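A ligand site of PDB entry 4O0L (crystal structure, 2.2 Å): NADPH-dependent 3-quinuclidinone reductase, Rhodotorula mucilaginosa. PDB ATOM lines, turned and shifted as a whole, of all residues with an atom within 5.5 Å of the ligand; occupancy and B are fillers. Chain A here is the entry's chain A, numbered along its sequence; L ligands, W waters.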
ATOM      1  N   GLY A  38     -22.187   3.210  12.176  1.00  0.00           N
ATOM      2  CA  GLY A  38     -22.372   3.900  10.889  1.00  0.00           C
ATOM      3  C   GLY A  38     -23.681   4.667  10.910  1.00  0.00           C
ATOM      4  O   GLY A  38     -24.294   4.895   9.868  1.00  0.00           O
ATOM      5  N   GLY A  39     -24.102   5.068  12.109  1.00  0.00           N
ATOM      6  CA  GLY A  39     -25.428   5.677  12.325  1.00  0.00           C
ATOM      7  C   GLY A  39     -25.589   7.044  11.672  1.00  0.00           C
ATOM      8  O   GLY A  39     -26.691   7.494  11.460  1.00  0.00           O
ATOM      9  N   GLY A  40     -24.488   7.705  11.384  1.00  0.00           N
ATOM     10  CA  GLY A  40     -24.516   8.968  10.599  1.00  0.00           C
ATOM     11  C   GLY A  40     -24.556   8.744   9.108  1.00  0.00           C
ATOM     12  O   GLY A  40     -24.802   9.674   8.358  1.00  0.00           O
ATOM     13  N   GLY A  41     -24.336   7.518   8.684  1.00  0.00           N
ATOM     14  CA  GLY A  41     -24.170   7.215   7.246  1.00  0.00           C
ATOM     15  C   GLY A  41     -25.502   6.918   6.566  1.00  0.00           C
ATOM     16  O   GLY A  41     -26.581   6.922   7.216  1.00  0.00           O
ATOM     17  N   GLY A  42     -25.437   6.663   5.253  1.00  0.00           N
ATOM     18  CA  GLY A  42     -26.633   6.425   4.433  1.00  0.00           C
ATOM     19  C   GLY A  42     -27.508   5.276   4.896  1.00  0.00           C
ATOM     20  O   GLY A  42     -28.644   5.474   5.298  1.00  0.00           O
ATOM     21  N   ILE A  43     -26.972   4.060   4.852  1.00  0.00           N
ATOM     22  CA  ILE A  43     -27.749   2.897   5.239  1.00  0.00           C
ATOM     23  C   ILE A  43     -28.118   2.928   6.748  1.00  0.00           C
ATOM     24  O   ILE A  43     -29.249   2.605   7.111  1.00  0.00           O
ATOM     25  CB  ILE A  43     -27.028   1.589   4.868  1.00  0.00           C
ATOM     26  CG1 ILE A  43     -26.890   1.505   3.332  1.00  0.00           C
ATOM     27  CG2 ILE A  43     -27.762   0.348   5.485  1.00  0.00           C
ATOM     28  CD1 ILE A  43     -26.038   0.336   2.903  1.00  0.00           C
ATOM     29  N   GLY A  44     -27.169   3.334   7.596  1.00  0.00           N
ATOM     30  CA  GLY A  44     -27.341   3.272   9.031  1.00  0.00           C
ATOM     31  C   GLY A  44     -28.424   4.194   9.543  1.00  0.00           C
ATOM     32  O   GLY A  44     -29.195   3.828  10.433  1.00  0.00           O
ATOM     33  N   TYR A  62     -21.346   6.620  15.867  1.00  0.00           N
ATOM     34  CA  TYR A  62     -20.701   7.373  14.789  1.00  0.00           C
ATOM     35  C   TYR A  62     -19.246   7.570  15.211  1.00  0.00           C
ATOM     36  O   TYR A  62     -18.927   7.432  16.401  1.00  0.00           O
ATOM     37  CB  TYR A  62     -21.355   8.749  14.584  1.00  0.00           C
ATOM     38  CG  TYR A  62     -21.085   9.718  15.761  1.00  0.00           C
ATOM     39  CD1 TYR A  62     -21.892   9.651  16.924  1.00  0.00           C
ATOM     40  CD2 TYR A  62     -20.038  10.617  15.734  1.00  0.00           C
ATOM     41  CE1 TYR A  62     -21.649  10.490  18.014  1.00  0.00           C
ATOM     42  CE2 TYR A  62     -19.785  11.473  16.813  1.00  0.00           C
ATOM     43  CZ  TYR A  62     -20.591  11.395  17.968  1.00  0.00           C
ATOM     44  OH  TYR A  62     -20.357  12.212  19.052  1.00  0.00           O
ATOM     45  N   ARG A  63     -18.398   7.920  14.237  1.00  0.00           N
ATOM     46  CA  ARG A  63     -16.991   8.200  14.471  1.00  0.00           C
ATOM     47  C   ARG A  63     -16.662   9.666  14.151  1.00  0.00           C
ATOM     48  O   ARG A  63     -16.223  10.415  15.032  1.00  0.00           O
ATOM     49  CB  ARG A  63     -16.125   7.258  13.632  1.00  0.00           C
ATOM     50  CG  ARG A  63     -14.628   7.575  13.636  1.00  0.00           C
ATOM     51  CD  ARG A  63     -13.870   6.891  12.496  1.00  0.00           C
ATOM     52  NE  ARG A  63     -14.498   7.159  11.204  1.00  0.00           N
ATOM     53  CZ  ARG A  63     -13.993   6.814  10.014  1.00  0.00           C
ATOM     54  NH1 ARG A  63     -12.827   6.172   9.925  1.00  0.00           N
ATOM     55  NH2 ARG A  63     -14.667   7.118   8.901  1.00  0.00           N
ATOM     56  N   SER A  64     -16.865  10.073  12.893  1.00  0.00           N
ATOM     57  CA  SER A  64     -16.474  11.402  12.413  1.00  0.00           C
ATOM     58  C   SER A  64     -17.660  12.224  11.912  1.00  0.00           C
ATOM     59  O   SER A  64     -17.534  13.406  11.655  1.00  0.00           O
ATOM     60  CB  SER A  64     -15.406  11.269  11.291  1.00  0.00           C
ATOM     61  OG  SER A  64     -16.010  10.872  10.075  1.00  0.00           O
ATOM     62  N   ALA A  65     -18.824  11.583  11.786  1.00  0.00           N
ATOM     63  CA  ALA A  65     -20.038  12.262  11.326  1.00  0.00           C
ATOM     64  C   ALA A  65     -20.330  13.516  12.181  1.00  0.00           C
ATOM     65  O   ALA A  65     -20.256  13.446  13.415  1.00  0.00           O
ATOM     66  CB  ALA A  65     -21.242  11.332  11.320  1.00  0.00           C
ATOM     67  N   CYS A  88     -18.042   6.113  18.659  1.00  0.00           N
ATOM     68  CA  CYS A  88     -17.506   4.763  18.668  1.00  0.00           C
ATOM     69  C   CYS A  88     -16.600   4.537  17.466  1.00  0.00           C
ATOM     70  O   CYS A  88     -17.018   4.684  16.323  1.00  0.00           O
ATOM     71  CB  CYS A  88     -18.659   3.735  18.691  1.00  0.00           C
ATOM     72  SG  CYS A  88     -18.107   2.014  18.599  1.00  0.00           S
ATOM     73  N   GLU A  89     -15.347   4.199  17.756  1.00  0.00           N
ATOM     74  CA  GLU A  89     -14.354   3.786  16.753  1.00  0.00           C
ATOM     75  C   GLU A  89     -14.394   2.272  16.664  1.00  0.00           C
ATOM     76  O   GLU A  89     -13.967   1.577  17.600  1.00  0.00           O
ATOM     77  CB  GLU A  89     -12.959   4.297  17.163  1.00  0.00           C
ATOM     78  CG  GLU A  89     -11.783   3.684  16.382  1.00  0.00           C
ATOM     79  CD  GLU A  89     -11.951   3.825  14.877  1.00  0.00           C
ATOM     80  OE1 GLU A  89     -12.089   4.967  14.355  1.00  0.00           O
ATOM     81  OE2 GLU A  89     -11.955   2.771  14.199  1.00  0.00           O
ATOM     82  N   VAL A  90     -14.928   1.739  15.566  1.00  0.00           N
ATOM     83  CA  VAL A  90     -15.273   0.310  15.545  1.00  0.00           C
ATOM     84  C   VAL A  90     -14.053  -0.638  15.435  1.00  0.00           C
ATOM     85  O   VAL A  90     -14.202  -1.841  15.684  1.00  0.00           O
ATOM     86  CB  VAL A  90     -16.335  -0.052  14.477  1.00  0.00           C
ATOM     87  CG1 VAL A  90     -17.638   0.734  14.701  1.00  0.00           C
ATOM     88  CG2 VAL A  90     -15.790   0.096  13.062  1.00  0.00           C
ATOM     89  N   THR A  91     -12.881  -0.087  15.083  1.00  0.00           N
ATOM     90  CA  THR A  91     -11.677  -0.895  14.971  1.00  0.00           C
ATOM     91  C   THR A  91     -10.984  -1.060  16.326  1.00  0.00           C
ATOM     92  O   THR A  91      -9.968  -1.755  16.429  1.00  0.00           O
ATOM     93  CB  THR A  91     -10.657  -0.271  13.983  1.00  0.00           C
ATOM     94  OG1 THR A  91     -10.225   0.990  14.493  1.00  0.00           O
ATOM     95  CG2 THR A  91     -11.261  -0.085  12.625  1.00  0.00           C
ATOM     96  N   ASN A 116     -23.163  -2.018  11.304  1.00  0.00           N
ATOM     97  CA  ASN A 116     -23.310  -1.441   9.981  1.00  0.00           C
ATOM     98  C   ASN A 116     -22.097  -0.636   9.483  1.00  0.00           C
ATOM     99  O   ASN A 116     -21.928  -0.468   8.275  1.00  0.00           O
ATOM    100  CB  ASN A 116     -24.574  -0.573   9.960  1.00  0.00           C
ATOM    101  CG  ASN A 116     -24.708   0.251   8.706  1.00  0.00           C
ATOM    102  OD1 ASN A 116     -24.481   1.453   8.737  1.00  0.00           O
ATOM    103  ND2 ASN A 116     -25.085  -0.384   7.595  1.00  0.00           N
ATOM    104  N   ALA A 117     -21.243  -0.159  10.387  1.00  0.00           N
ATOM    105  CA  ALA A 117     -20.027   0.540   9.988  1.00  0.00           C
ATOM    106  C   ALA A 117     -19.147  -0.356   9.086  1.00  0.00           C
ATOM    107  O   ALA A 117     -19.042  -1.541   9.293  1.00  0.00           O
ATOM    108  CB  ALA A 117     -19.224   1.063  11.202  1.00  0.00           C
ATOM    109  N   GLY A 118     -18.515   0.252   8.087  1.00  0.00           N
ATOM    110  CA  GLY A 118     -17.675  -0.484   7.179  1.00  0.00           C
ATOM    111  C   GLY A 118     -16.863   0.475   6.351  1.00  0.00           C
ATOM    112  O   GLY A 118     -17.082   1.684   6.386  1.00  0.00           O
ATOM    113  N   GLY A 119     -15.926  -0.093   5.611  1.00  0.00           N
ATOM    114  CA  GLY A 119     -14.982   0.691   4.798  1.00  0.00           C
ATOM    115  C   GLY A 119     -13.876  -0.241   4.361  1.00  0.00           C
ATOM    116  O   GLY A 119     -14.097  -1.442   4.244  1.00  0.00           O
ATOM    117  N   LYS A 136      -6.429  -2.736   8.207  1.00  0.00           N
ATOM    118  CA  LYS A 136      -7.469  -1.713   8.411  1.00  0.00           C
ATOM    119  C   LYS A 136      -8.785  -2.217   7.873  1.00  0.00           C
ATOM    120  O   LYS A 136      -9.804  -2.174   8.578  1.00  0.00           O
ATOM    121  CB  LYS A 136      -7.078  -0.336   7.828  1.00  0.00           C
ATOM    122  CG  LYS A 136      -8.240   0.674   7.745  1.00  0.00           C
ATOM    123  CD  LYS A 136      -8.786   1.235   9.107  1.00  0.00           C
ATOM    124  CE  LYS A 136      -8.091   2.577   9.497  1.00  0.00           C
ATOM    125  NZ  LYS A 136      -8.804   3.521  10.459  1.00  0.00           N
ATOM    126  N   VAL A 140     -12.108  -2.897  10.219  1.00  0.00           N
ATOM    127  CA  VAL A 140     -13.292  -2.064  10.128  1.00  0.00           C
ATOM    128  C   VAL A 140     -14.565  -2.902   9.835  1.00  0.00           C
ATOM    129  O   VAL A 140     -15.668  -2.604  10.366  1.00  0.00           O
ATOM    130  CB  VAL A 140     -13.067  -0.868   9.150  1.00  0.00           C
ATOM    131  CG1 VAL A 140     -12.986  -1.336   7.699  1.00  0.00           C
ATOM    132  CG2 VAL A 140     -14.172   0.203   9.299  1.00  0.00           C
ATOM    133  N   ASN A 141     -14.424  -3.950   9.019  1.00  0.00           N
ATOM    134  CA  ASN A 141     -15.549  -4.806   8.646  1.00  0.00           C
ATOM    135  C   ASN A 141     -15.723  -6.024   9.557  1.00  0.00           C
ATOM    136  O   ASN A 141     -16.825  -6.271  10.058  1.00  0.00           O
ATOM    137  CB  ASN A 141     -15.441  -5.237   7.178  1.00  0.00           C
ATOM    138  CG  ASN A 141     -15.364  -4.032   6.236  1.00  0.00           C
ATOM    139  OD1 ASN A 141     -15.943  -2.985   6.500  1.00  0.00           O
ATOM    140  ND2 ASN A 141     -14.623  -4.186   5.124  1.00  0.00           N
ATOM    141  N   THR A 167     -24.368  -5.553   8.443  1.00  0.00           N
ATOM    142  CA  THR A 167     -24.468  -5.177   7.061  1.00  0.00           C
ATOM    143  C   THR A 167     -23.284  -5.763   6.339  1.00  0.00           C
ATOM    144  O   THR A 167     -22.173  -5.349   6.526  1.00  0.00           O
ATOM    145  CB  THR A 167     -24.476  -3.653   6.858  1.00  0.00           C
ATOM    146  OG1 THR A 167     -25.626  -3.121   7.510  1.00  0.00           O
ATOM    147  CG2 THR A 167     -24.548  -3.347   5.393  1.00  0.00           C
ATOM    148  N   THR A 168     -23.551  -6.749   5.501  1.00  0.00           N
ATOM    149  CA  THR A 168     -22.482  -7.329   4.695  1.00  0.00           C
ATOM    150  C   THR A 168     -22.513  -6.675   3.316  1.00  0.00           C
ATOM    151  O   THR A 168     -22.579  -5.426   3.227  1.00  0.00           O
ATOM    152  CB  THR A 168     -22.534  -8.861   4.715  1.00  0.00           C
ATOM    153  OG1 THR A 168     -23.894  -9.310   4.584  1.00  0.00           O
ATOM    154  CG2 THR A 168     -22.050  -9.343   6.058  1.00  0.00           C
ATOM    155  N   SER A 169     -22.495  -7.458   2.251  1.00  0.00           N
ATOM    156  CA  SER A 169     -22.481  -6.884   0.912  1.00  0.00           C
ATOM    157  C   SER A 169     -22.563  -8.018  -0.105  1.00  0.00           C
ATOM    158  O   SER A 169     -22.274  -9.182   0.222  1.00  0.00           O
ATOM    159  CB  SER A 169     -21.231  -6.035   0.705  1.00  0.00           C
ATOM    160  OG  SER A 169     -20.890  -5.800  -0.642  1.00  0.00           O
ATOM    161  N   ILE A 170     -22.988  -7.689  -1.319  1.00  0.00           N
ATOM    162  CA  ILE A 170     -22.791  -8.545  -2.473  1.00  0.00           C
ATOM    163  C   ILE A 170     -21.328  -8.989  -2.588  1.00  0.00           C
ATOM    164  O   ILE A 170     -21.043 -10.068  -3.105  1.00  0.00           O
ATOM    165  CB  ILE A 170     -23.191  -7.852  -3.806  1.00  0.00           C
ATOM    166  CG1 ILE A 170     -22.546  -6.454  -3.940  1.00  0.00           C
ATOM    167  CG2 ILE A 170     -24.708  -7.793  -3.956  1.00  0.00           C
ATOM    168  CD1 ILE A 170     -22.603  -5.855  -5.364  1.00  0.00           C
ATOM    169  N   TYR A 184     -11.519  -6.282   1.156  1.00  0.00           N
ATOM    170  CA  TYR A 184     -12.897  -5.943   1.492  1.00  0.00           C
ATOM    171  C   TYR A 184     -13.809  -7.111   1.217  1.00  0.00           C
ATOM    172  O   TYR A 184     -14.670  -7.415   2.032  1.00  0.00           O
ATOM    173  CB  TYR A 184     -13.335  -4.715   0.687  1.00  0.00           C
ATOM    174  CG  TYR A 184     -14.749  -4.255   0.914  1.00  0.00           C
ATOM    175  CD1 TYR A 184     -15.795  -4.775   0.150  1.00  0.00           C
ATOM    176  CD2 TYR A 184     -15.049  -3.264   1.841  1.00  0.00           C
ATOM    177  CE1 TYR A 184     -17.097  -4.342   0.332  1.00  0.00           C
ATOM    178  CE2 TYR A 184     -16.341  -2.832   2.050  1.00  0.00           C
ATOM    179  CZ  TYR A 184     -17.374  -3.371   1.287  1.00  0.00           C
ATOM    180  OH  TYR A 184     -18.682  -2.937   1.456  1.00  0.00           O
ATOM    181  N   LYS A 188     -16.063  -9.140   4.309  1.00  0.00           N
ATOM    182  CA  LYS A 188     -17.531  -9.285   4.273  1.00  0.00           C
ATOM    183  C   LYS A 188     -18.003 -10.747   4.223  1.00  0.00           C
ATOM    184  O   LYS A 188     -19.017 -11.081   4.845  1.00  0.00           O
ATOM    185  CB  LYS A 188     -18.106  -8.513   3.094  1.00  0.00           C
ATOM    186  CG  LYS A 188     -17.897  -6.980   3.173  1.00  0.00           C
ATOM    187  CD  LYS A 188     -18.659  -6.361   4.341  1.00  0.00           C
ATOM    188  CE  LYS A 188     -18.702  -4.829   4.236  1.00  0.00           C
ATOM    189  NZ  LYS A 188     -19.533  -4.179   5.311  1.00  0.00           N
ATOM    190  N   PRO A 213     -26.393  -5.675   0.977  1.00  0.00           N
ATOM    191  CA  PRO A 213     -26.851  -4.766  -0.087  1.00  0.00           C
ATOM    192  C   PRO A 213     -25.979  -4.935  -1.356  1.00  0.00           C
ATOM    193  O   PRO A 213     -24.804  -5.280  -1.265  1.00  0.00           O
ATOM    194  CB  PRO A 213     -26.628  -3.371   0.510  1.00  0.00           C
ATOM    195  CG  PRO A 213     -26.367  -3.578   1.976  1.00  0.00           C
ATOM    196  CD  PRO A 213     -25.713  -4.940   2.053  1.00  0.00           C
ATOM    197  N   GLY A 214     -26.589  -4.712  -2.513  1.00  0.00           N
ATOM    198  CA  GLY A 214     -25.867  -4.439  -3.746  1.00  0.00           C
ATOM    199  C   GLY A 214     -25.417  -3.015  -3.667  1.00  0.00           C
ATOM    200  O   GLY A 214     -25.264  -2.481  -2.567  1.00  0.00           O
ATOM    201  N   PHE A 215     -25.162  -2.375  -4.815  1.00  0.00           N
ATOM    202  CA  PHE A 215     -24.732  -0.972  -4.805  1.00  0.00           C
ATOM    203  C   PHE A 215     -25.886  -0.046  -4.433  1.00  0.00           C
ATOM    204  O   PHE A 215     -26.991  -0.146  -4.970  1.00  0.00           O
ATOM    205  CB  PHE A 215     -24.185  -0.564  -6.169  1.00  0.00           C
ATOM    206  CG  PHE A 215     -22.835  -1.138  -6.468  1.00  0.00           C
ATOM    207  CD1 PHE A 215     -21.673  -0.502  -6.007  1.00  0.00           C
ATOM    208  CD2 PHE A 215     -22.710  -2.302  -7.208  1.00  0.00           C
ATOM    209  CE1 PHE A 215     -20.415  -1.028  -6.292  1.00  0.00           C
ATOM    210  CE2 PHE A 215     -21.440  -2.835  -7.483  1.00  0.00           C
ATOM    211  CZ  PHE A 215     -20.307  -2.214  -7.027  1.00  0.00           C
ATOM    212  N   PHE A 216     -25.612   0.875  -3.541  1.00  0.00           N
ATOM    213  CA  PHE A 216     -26.573   1.869  -3.125  1.00  0.00           C
ATOM    214  C   PHE A 216     -25.995   3.249  -3.250  1.00  0.00           C
ATOM    215  O   PHE A 216     -24.783   3.440  -3.113  1.00  0.00           O
ATOM    216  CB  PHE A 216     -27.045   1.615  -1.684  1.00  0.00           C
ATOM    217  CG  PHE A 216     -28.193   0.672  -1.598  1.00  0.00           C
ATOM    218  CD1 PHE A 216     -28.004  -0.688  -1.812  1.00  0.00           C
ATOM    219  CD2 PHE A 216     -29.460   1.134  -1.298  1.00  0.00           C
ATOM    220  CE1 PHE A 216     -29.075  -1.580  -1.722  1.00  0.00           C
ATOM    221  CE2 PHE A 216     -30.538   0.266  -1.242  1.00  0.00           C
ATOM    222  CZ  PHE A 216     -30.349  -1.093  -1.457  1.00  0.00           C
ATOM    223  N   ASP A 217     -26.880   4.214  -3.517  1.00  0.00           N
ATOM    224  CA  ASP A 217     -26.526   5.597  -3.639  1.00  0.00           C
ATOM    225  C   ASP A 217     -26.181   6.190  -2.253  1.00  0.00           C
ATOM    226  O   ASP A 217     -27.030   6.704  -1.558  1.00  0.00           O
ATOM    227  CB  ASP A 217     -27.708   6.347  -4.305  1.00  0.00           C
ATOM    228  CG  ASP A 217     -27.465   7.858  -4.461  1.00  0.00           C
ATOM    229  OD1 ASP A 217     -26.306   8.295  -4.472  1.00  0.00           O
ATOM    230  OD2 ASP A 217     -28.472   8.583  -4.603  1.00  0.00           O
ATOM    231  N   THR A 218     -24.911   6.057  -1.861  1.00  0.00           N
ATOM    232  CA  THR A 218     -24.374   6.575  -0.597  1.00  0.00           C
ATOM    233  C   THR A 218     -22.914   6.895  -0.913  1.00  0.00           C
ATOM    234  O   THR A 218     -22.472   6.589  -2.002  1.00  0.00           O
ATOM    235  CB  THR A 218     -24.405   5.525   0.556  1.00  0.00           C
ATOM    236  OG1 THR A 218     -23.390   4.540   0.348  1.00  0.00           O
ATOM    237  CG2 THR A 218     -25.759   4.855   0.705  1.00  0.00           C
ATOM    238  N   PRO A 219     -22.165   7.521   0.024  1.00  0.00           N
ATOM    239  CA  PRO A 219     -20.727   7.750  -0.251  1.00  0.00           C
ATOM    240  C   PRO A 219     -19.922   6.472  -0.492  1.00  0.00           C
ATOM    241  O   PRO A 219     -18.788   6.548  -0.984  1.00  0.00           O
ATOM    242  CB  PRO A 219     -20.230   8.458   1.015  1.00  0.00           C
ATOM    243  CG  PRO A 219     -21.474   9.104   1.604  1.00  0.00           C
ATOM    244  CD  PRO A 219     -22.565   8.098   1.331  1.00  0.00           C
ATOM    245  N   MET A 220     -20.486   5.313  -0.179  1.00  0.00           N
ATOM    246  CA  MET A 220     -19.818   4.043  -0.459  1.00  0.00           C
ATOM    247  C   MET A 220     -20.392   3.331  -1.696  1.00  0.00           C
ATOM    248  O   MET A 220     -20.101   2.159  -1.939  1.00  0.00           O
ATOM    249  CB  MET A 220     -19.885   3.128   0.783  1.00  0.00           C
ATOM    250  CG  MET A 220     -18.986   3.597   1.905  1.00  0.00           C
ATOM    251  SD  MET A 220     -18.713   2.325   3.142  1.00  0.00           S
ATOM    252  CE  MET A 220     -17.787   1.095   2.196  1.00  0.00           C
ATOM    253  N   GLY A 221     -21.207   4.054  -2.474  1.00  0.00           N
ATOM    254  CA  GLY A 221     -21.745   3.530  -3.729  1.00  0.00           C
ATOM    255  C   GLY A 221     -20.705   3.550  -4.847  1.00  0.00           C
ATOM    256  O   GLY A 221     -19.519   3.683  -4.583  1.00  0.00           O
ATOM    257  N   PRO A 222     -21.143   3.388  -6.106  1.00  0.00           N
ATOM    258  CA  PRO A 222     -20.165   3.270  -7.239  1.00  0.00           C
ATOM    259  C   PRO A 222     -19.115   4.395  -7.278  1.00  0.00           C
ATOM    260  O   PRO A 222     -19.467   5.555  -7.346  1.00  0.00           O
ATOM    261  CB  PRO A 222     -21.057   3.272  -8.482  1.00  0.00           C
ATOM    262  CG  PRO A 222     -22.399   2.786  -7.970  1.00  0.00           C
ATOM    263  CD  PRO A 222     -22.533   3.336  -6.584  1.00  0.00           C
HETATM  264  P1  LIG L   1     -21.653   5.655   4.337  1.00  0.00           P
HETATM  265  O1  LIG L   1     -20.399   6.157   3.754  1.00  0.00           O
HETATM  266  O2  LIG L   1     -22.772   6.625   4.372  1.00  0.00           O
HETATM  267  O3  LIG L   1     -21.448   4.967   5.768  1.00  0.00           O
HETATM  268  C1  LIG L   1     -20.242   4.324   6.165  1.00  0.00           C
HETATM  269  C2  LIG L   1     -20.251   4.448   7.685  1.00  0.00           C
HETATM  270  O4  LIG L   1     -19.203   3.717   8.297  1.00  0.00           O
HETATM  271  C3  LIG L   1     -20.093   5.899   8.082  1.00  0.00           C
HETATM  272  O5  LIG L   1     -21.270   6.235   8.787  1.00  0.00           O
HETATM  273  C4  LIG L   1     -18.863   5.953   8.940  1.00  0.00           C
HETATM  274  O6  LIG L   1     -19.067   6.700  10.113  1.00  0.00           O
HETATM  275  C5  LIG L   1     -18.655   4.500   9.327  1.00  0.00           C
HETATM  276  N1  LIG L   1     -17.244   4.118   9.584  1.00  0.00           N
HETATM  277  C6  LIG L   1     -16.252   3.844   8.680  1.00  0.00           C
HETATM  278  N2  LIG L   1     -15.122   3.522   9.343  1.00  0.00           N
HETATM  279  C7  LIG L   1     -15.399   3.566  10.643  1.00  0.00           C
HETATM  280  C8  LIG L   1     -14.648   3.335  11.813  1.00  0.00           C
HETATM  281  N3  LIG L   1     -13.382   2.973  11.725  1.00  0.00           N
HETATM  282  N4  LIG L   1     -15.248   3.497  13.038  1.00  0.00           N
HETATM  283  C9  LIG L   1     -16.547   3.878  13.171  1.00  0.00           C
HETATM  284  N5  LIG L   1     -17.297   4.120  12.046  1.00  0.00           N
HETATM  285  C10 LIG L   1     -16.748   3.962  10.826  1.00  0.00           C
HETATM  286  O7  LIG L   1     -22.029   4.392   3.374  1.00  0.00           O
HETATM  287  P2  LIG L   1     -23.089   3.206   3.580  1.00  0.00           P
HETATM  288  O8  LIG L   1     -23.359   2.711   2.193  1.00  0.00           O
HETATM  289  O9  LIG L   1     -24.169   3.669   4.475  1.00  0.00           O
HETATM  290  O10 LIG L   1     -22.214   2.043   4.341  1.00  0.00           O
HETATM  291  C11 LIG L   1     -22.761   1.332   5.423  1.00  0.00           C
HETATM  292  C12 LIG L   1     -22.438  -0.163   5.279  1.00  0.00           C
HETATM  293  O11 LIG L   1     -22.995  -0.721   4.082  1.00  0.00           O
HETATM  294  C13 LIG L   1     -20.943  -0.466   5.234  1.00  0.00           C
HETATM  295  O12 LIG L   1     -20.782  -1.591   6.037  1.00  0.00           O
HETATM  296  C14 LIG L   1     -20.670  -0.854   3.797  1.00  0.00           C
HETATM  297  O13 LIG L   1     -19.616  -1.788   3.735  1.00  0.00           O
HETATM  298  C15 LIG L   1     -22.002  -1.493   3.409  1.00  0.00           C
HETATM  299  N6  LIG L   1     -22.330  -1.546   1.977  1.00  0.00           N
HETATM  300  C16 LIG L   1     -22.464  -0.418   1.233  1.00  0.00           C
HETATM  301  C17 LIG L   1     -22.786  -0.514  -0.128  1.00  0.00           C
HETATM  302  C18 LIG L   1     -23.078   0.678  -1.013  1.00  0.00           C
HETATM  303  O14 LIG L   1     -23.144   0.493  -2.317  1.00  0.00           O
HETATM  304  N7  LIG L   1     -23.325   1.868  -0.444  1.00  0.00           N
HETATM  305  C19 LIG L   1     -23.016  -1.805  -0.701  1.00  0.00           C
HETATM  306  C20 LIG L   1     -22.891  -2.950   0.092  1.00  0.00           C
HETATM  307  C21 LIG L   1     -22.554  -2.797   1.434  1.00  0.00           C
HETATM  308  P3  LIG L   1     -18.487   8.190  10.320  1.00  0.00           P
HETATM  309  O15 LIG L   1     -19.138   8.710  11.591  1.00  0.00           O
HETATM  310  O16 LIG L   1     -16.989   8.174  10.434  1.00  0.00           O
HETATM  311  O17 LIG L   1     -18.876   8.995   9.170  1.00  0.00           O
HETATM  312  O   HOH W   1     -21.441   7.224  11.462  1.00  0.00           O
HETATM  313  O   HOH W   2     -18.746  11.770   8.035  1.00  0.00           O
HETATM  314  O   HOH W   3     -24.324   3.919   7.195  1.00  0.00           O
HETATM  315  O   HOH W   4     -10.800   5.235  12.016  1.00  0.00           O
HETATM  316  O   HOH W   5     -19.922  -3.147  -0.999  1.00  0.00           O
HETATM  317  O   HOH W   6     -12.880   3.328   7.714  1.00  0.00           O
HETATM  318  O   HOH W   7     -20.019   4.849  12.850  1.00  0.00           O
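The backbone NH of Arg 63 sits at hydrogen-bond distance from an oxygen (O15) of the ligand.
OH of Tyr 184 sits at hydrogen-bond distance from O13 of the ligand, 2.7 Å away.
A nitrogen (N3) of the ligand sits at hydrogen-bond distance from the side-chain carboxylate of Glu 89 (2.9 Å).
An oxygen (O12) of the ligand lies within hydrogen-bond range of the backbone carbonyl oxygen of Asn 116.
NE of Arg 63 is in salt-bridge range of O16 of the ligand (2.8 Å).
N of Val 90 lies within hydrogen-bond range of N4 of the ligand (3.1 Å).
NZ of Lys 188 lies within hydrogen-bond range of O13 of the ligand.
O5 of the ligand lies within hydrogen-bond range of N of Gly 41 (3.3 Å).
The backbone NH of Gly 42 sits at hydrogen-bond distance from an oxygen (O2) of the ligand (2.8 Å).
O of Phe 216 lies within hydrogen-bond range of N7 of the ligand (3.4 Å).
O8 of the ligand is in hydrogen-bond range of OG1 of Thr 218 (2.6 Å).
O9 of the ligand is in hydrogen-bond range of N of Ile 43 (2.9 Å).
The backbone NH (N) of Phe 216 sits at hydrogen-bond distance from an oxygen (O14) of the ligand (2.8 Å).
O16 of the ligand lies within hydrogen-bond range of OG of Ser 64, at 2.9 Å.
The backbone NH (N) of Ala 65 sits at hydrogen-bond distance from an oxygen (O15) of the ligand, at 2.9 Å.
N of Ser 64 is in hydrogen-bond range of O15 of the ligand.
The backbone carbonyl oxygen (O) of Gly 38 lies close to an oxygen (O5) of the ligand, at 3.5 Å.
OD1 of Asn 116 sits close to N of Gly 44 (3.5 Å).
The backbone carbonyl oxygen (O) of Pro 213 is in hydrogen-bond range of the backbone NH (N) of Ile 170 (3.0 Å).
The backbone carbonyl oxygen of Thr 167 sits at hydrogen-bond distance from the side-chain amino group of Lys 188.
OG1 of Thr 218 sits close to N of Met 220 (3.1 Å).
ND2 of Asn 116 sits at hydrogen-bond distance from OG1 of Thr 167 (2.8 Å).
N of Cys 88 is in hydrogen-bond range of O of Tyr 62 (2.8 Å).
OG1 of Thr 91 is in hydrogen-bond range of OE2 of Glu 89 (2.5 Å).
The backbone carbonyl oxygen (O) of Met 220 lies close to an oxygen (O14) of the ligand (3.5 Å).
Merely in contact with the ligand: Gly 214, Thr 168, Gly 118, Cys 88, Phe 215, Pro 213, Thr 167, Pro 219, Val 140, Ser 169, Gly 221, Ala 117, Tyr 62 and Thr 91.
Within 4 Å of the ligand: Gly 38, Gly 41, Gly 42, Ile 43, Tyr 62, Arg 63, Ser 64, Ala 65, Cys 88, Glu 89, Val 90, Thr 91, Asn 116, Ala 117, Gly 118, Val 140, Thr 167, Thr 168, Ser 169, Tyr 184, Lys 188, Pro 213, Gly 214, Phe 215, Phe 216, Thr 218, Pro 219, Met 220 and Gly 221.
Along chain A the residues within 4 Å of the ligand span positions 38 to 221.
The nearest printed residue that does not touch the ligand is Gly 40 (4.1 Å).
Water W3 lies within hydrogen-bond range of an oxygen (O9) of the ligand (2.7 Å), the backbone carbonyl oxygen (O) of Gly 38 (2.8 Å), the side-chain amide oxygen (OD1) of Asn 116 (2.9 Å) and the backbone NH (N) of Gly 44 (2.9 Å).
Water W1 lies within hydrogen-bond range of an oxygen (O15) of the ligand (2.7 Å), the backbone NH of Gly 40 (3.1 Å) and the backbone NH of Gly 39 (3.5 Å).
Water W7 bridges N of Gly 38 (2.8 Å) and N5 of the ligand (2.9 Å).
Water W5 lies within hydrogen-bond range of OH of Tyr 184 (2.8 Å) and OG of Ser 169 (2.8 Å).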
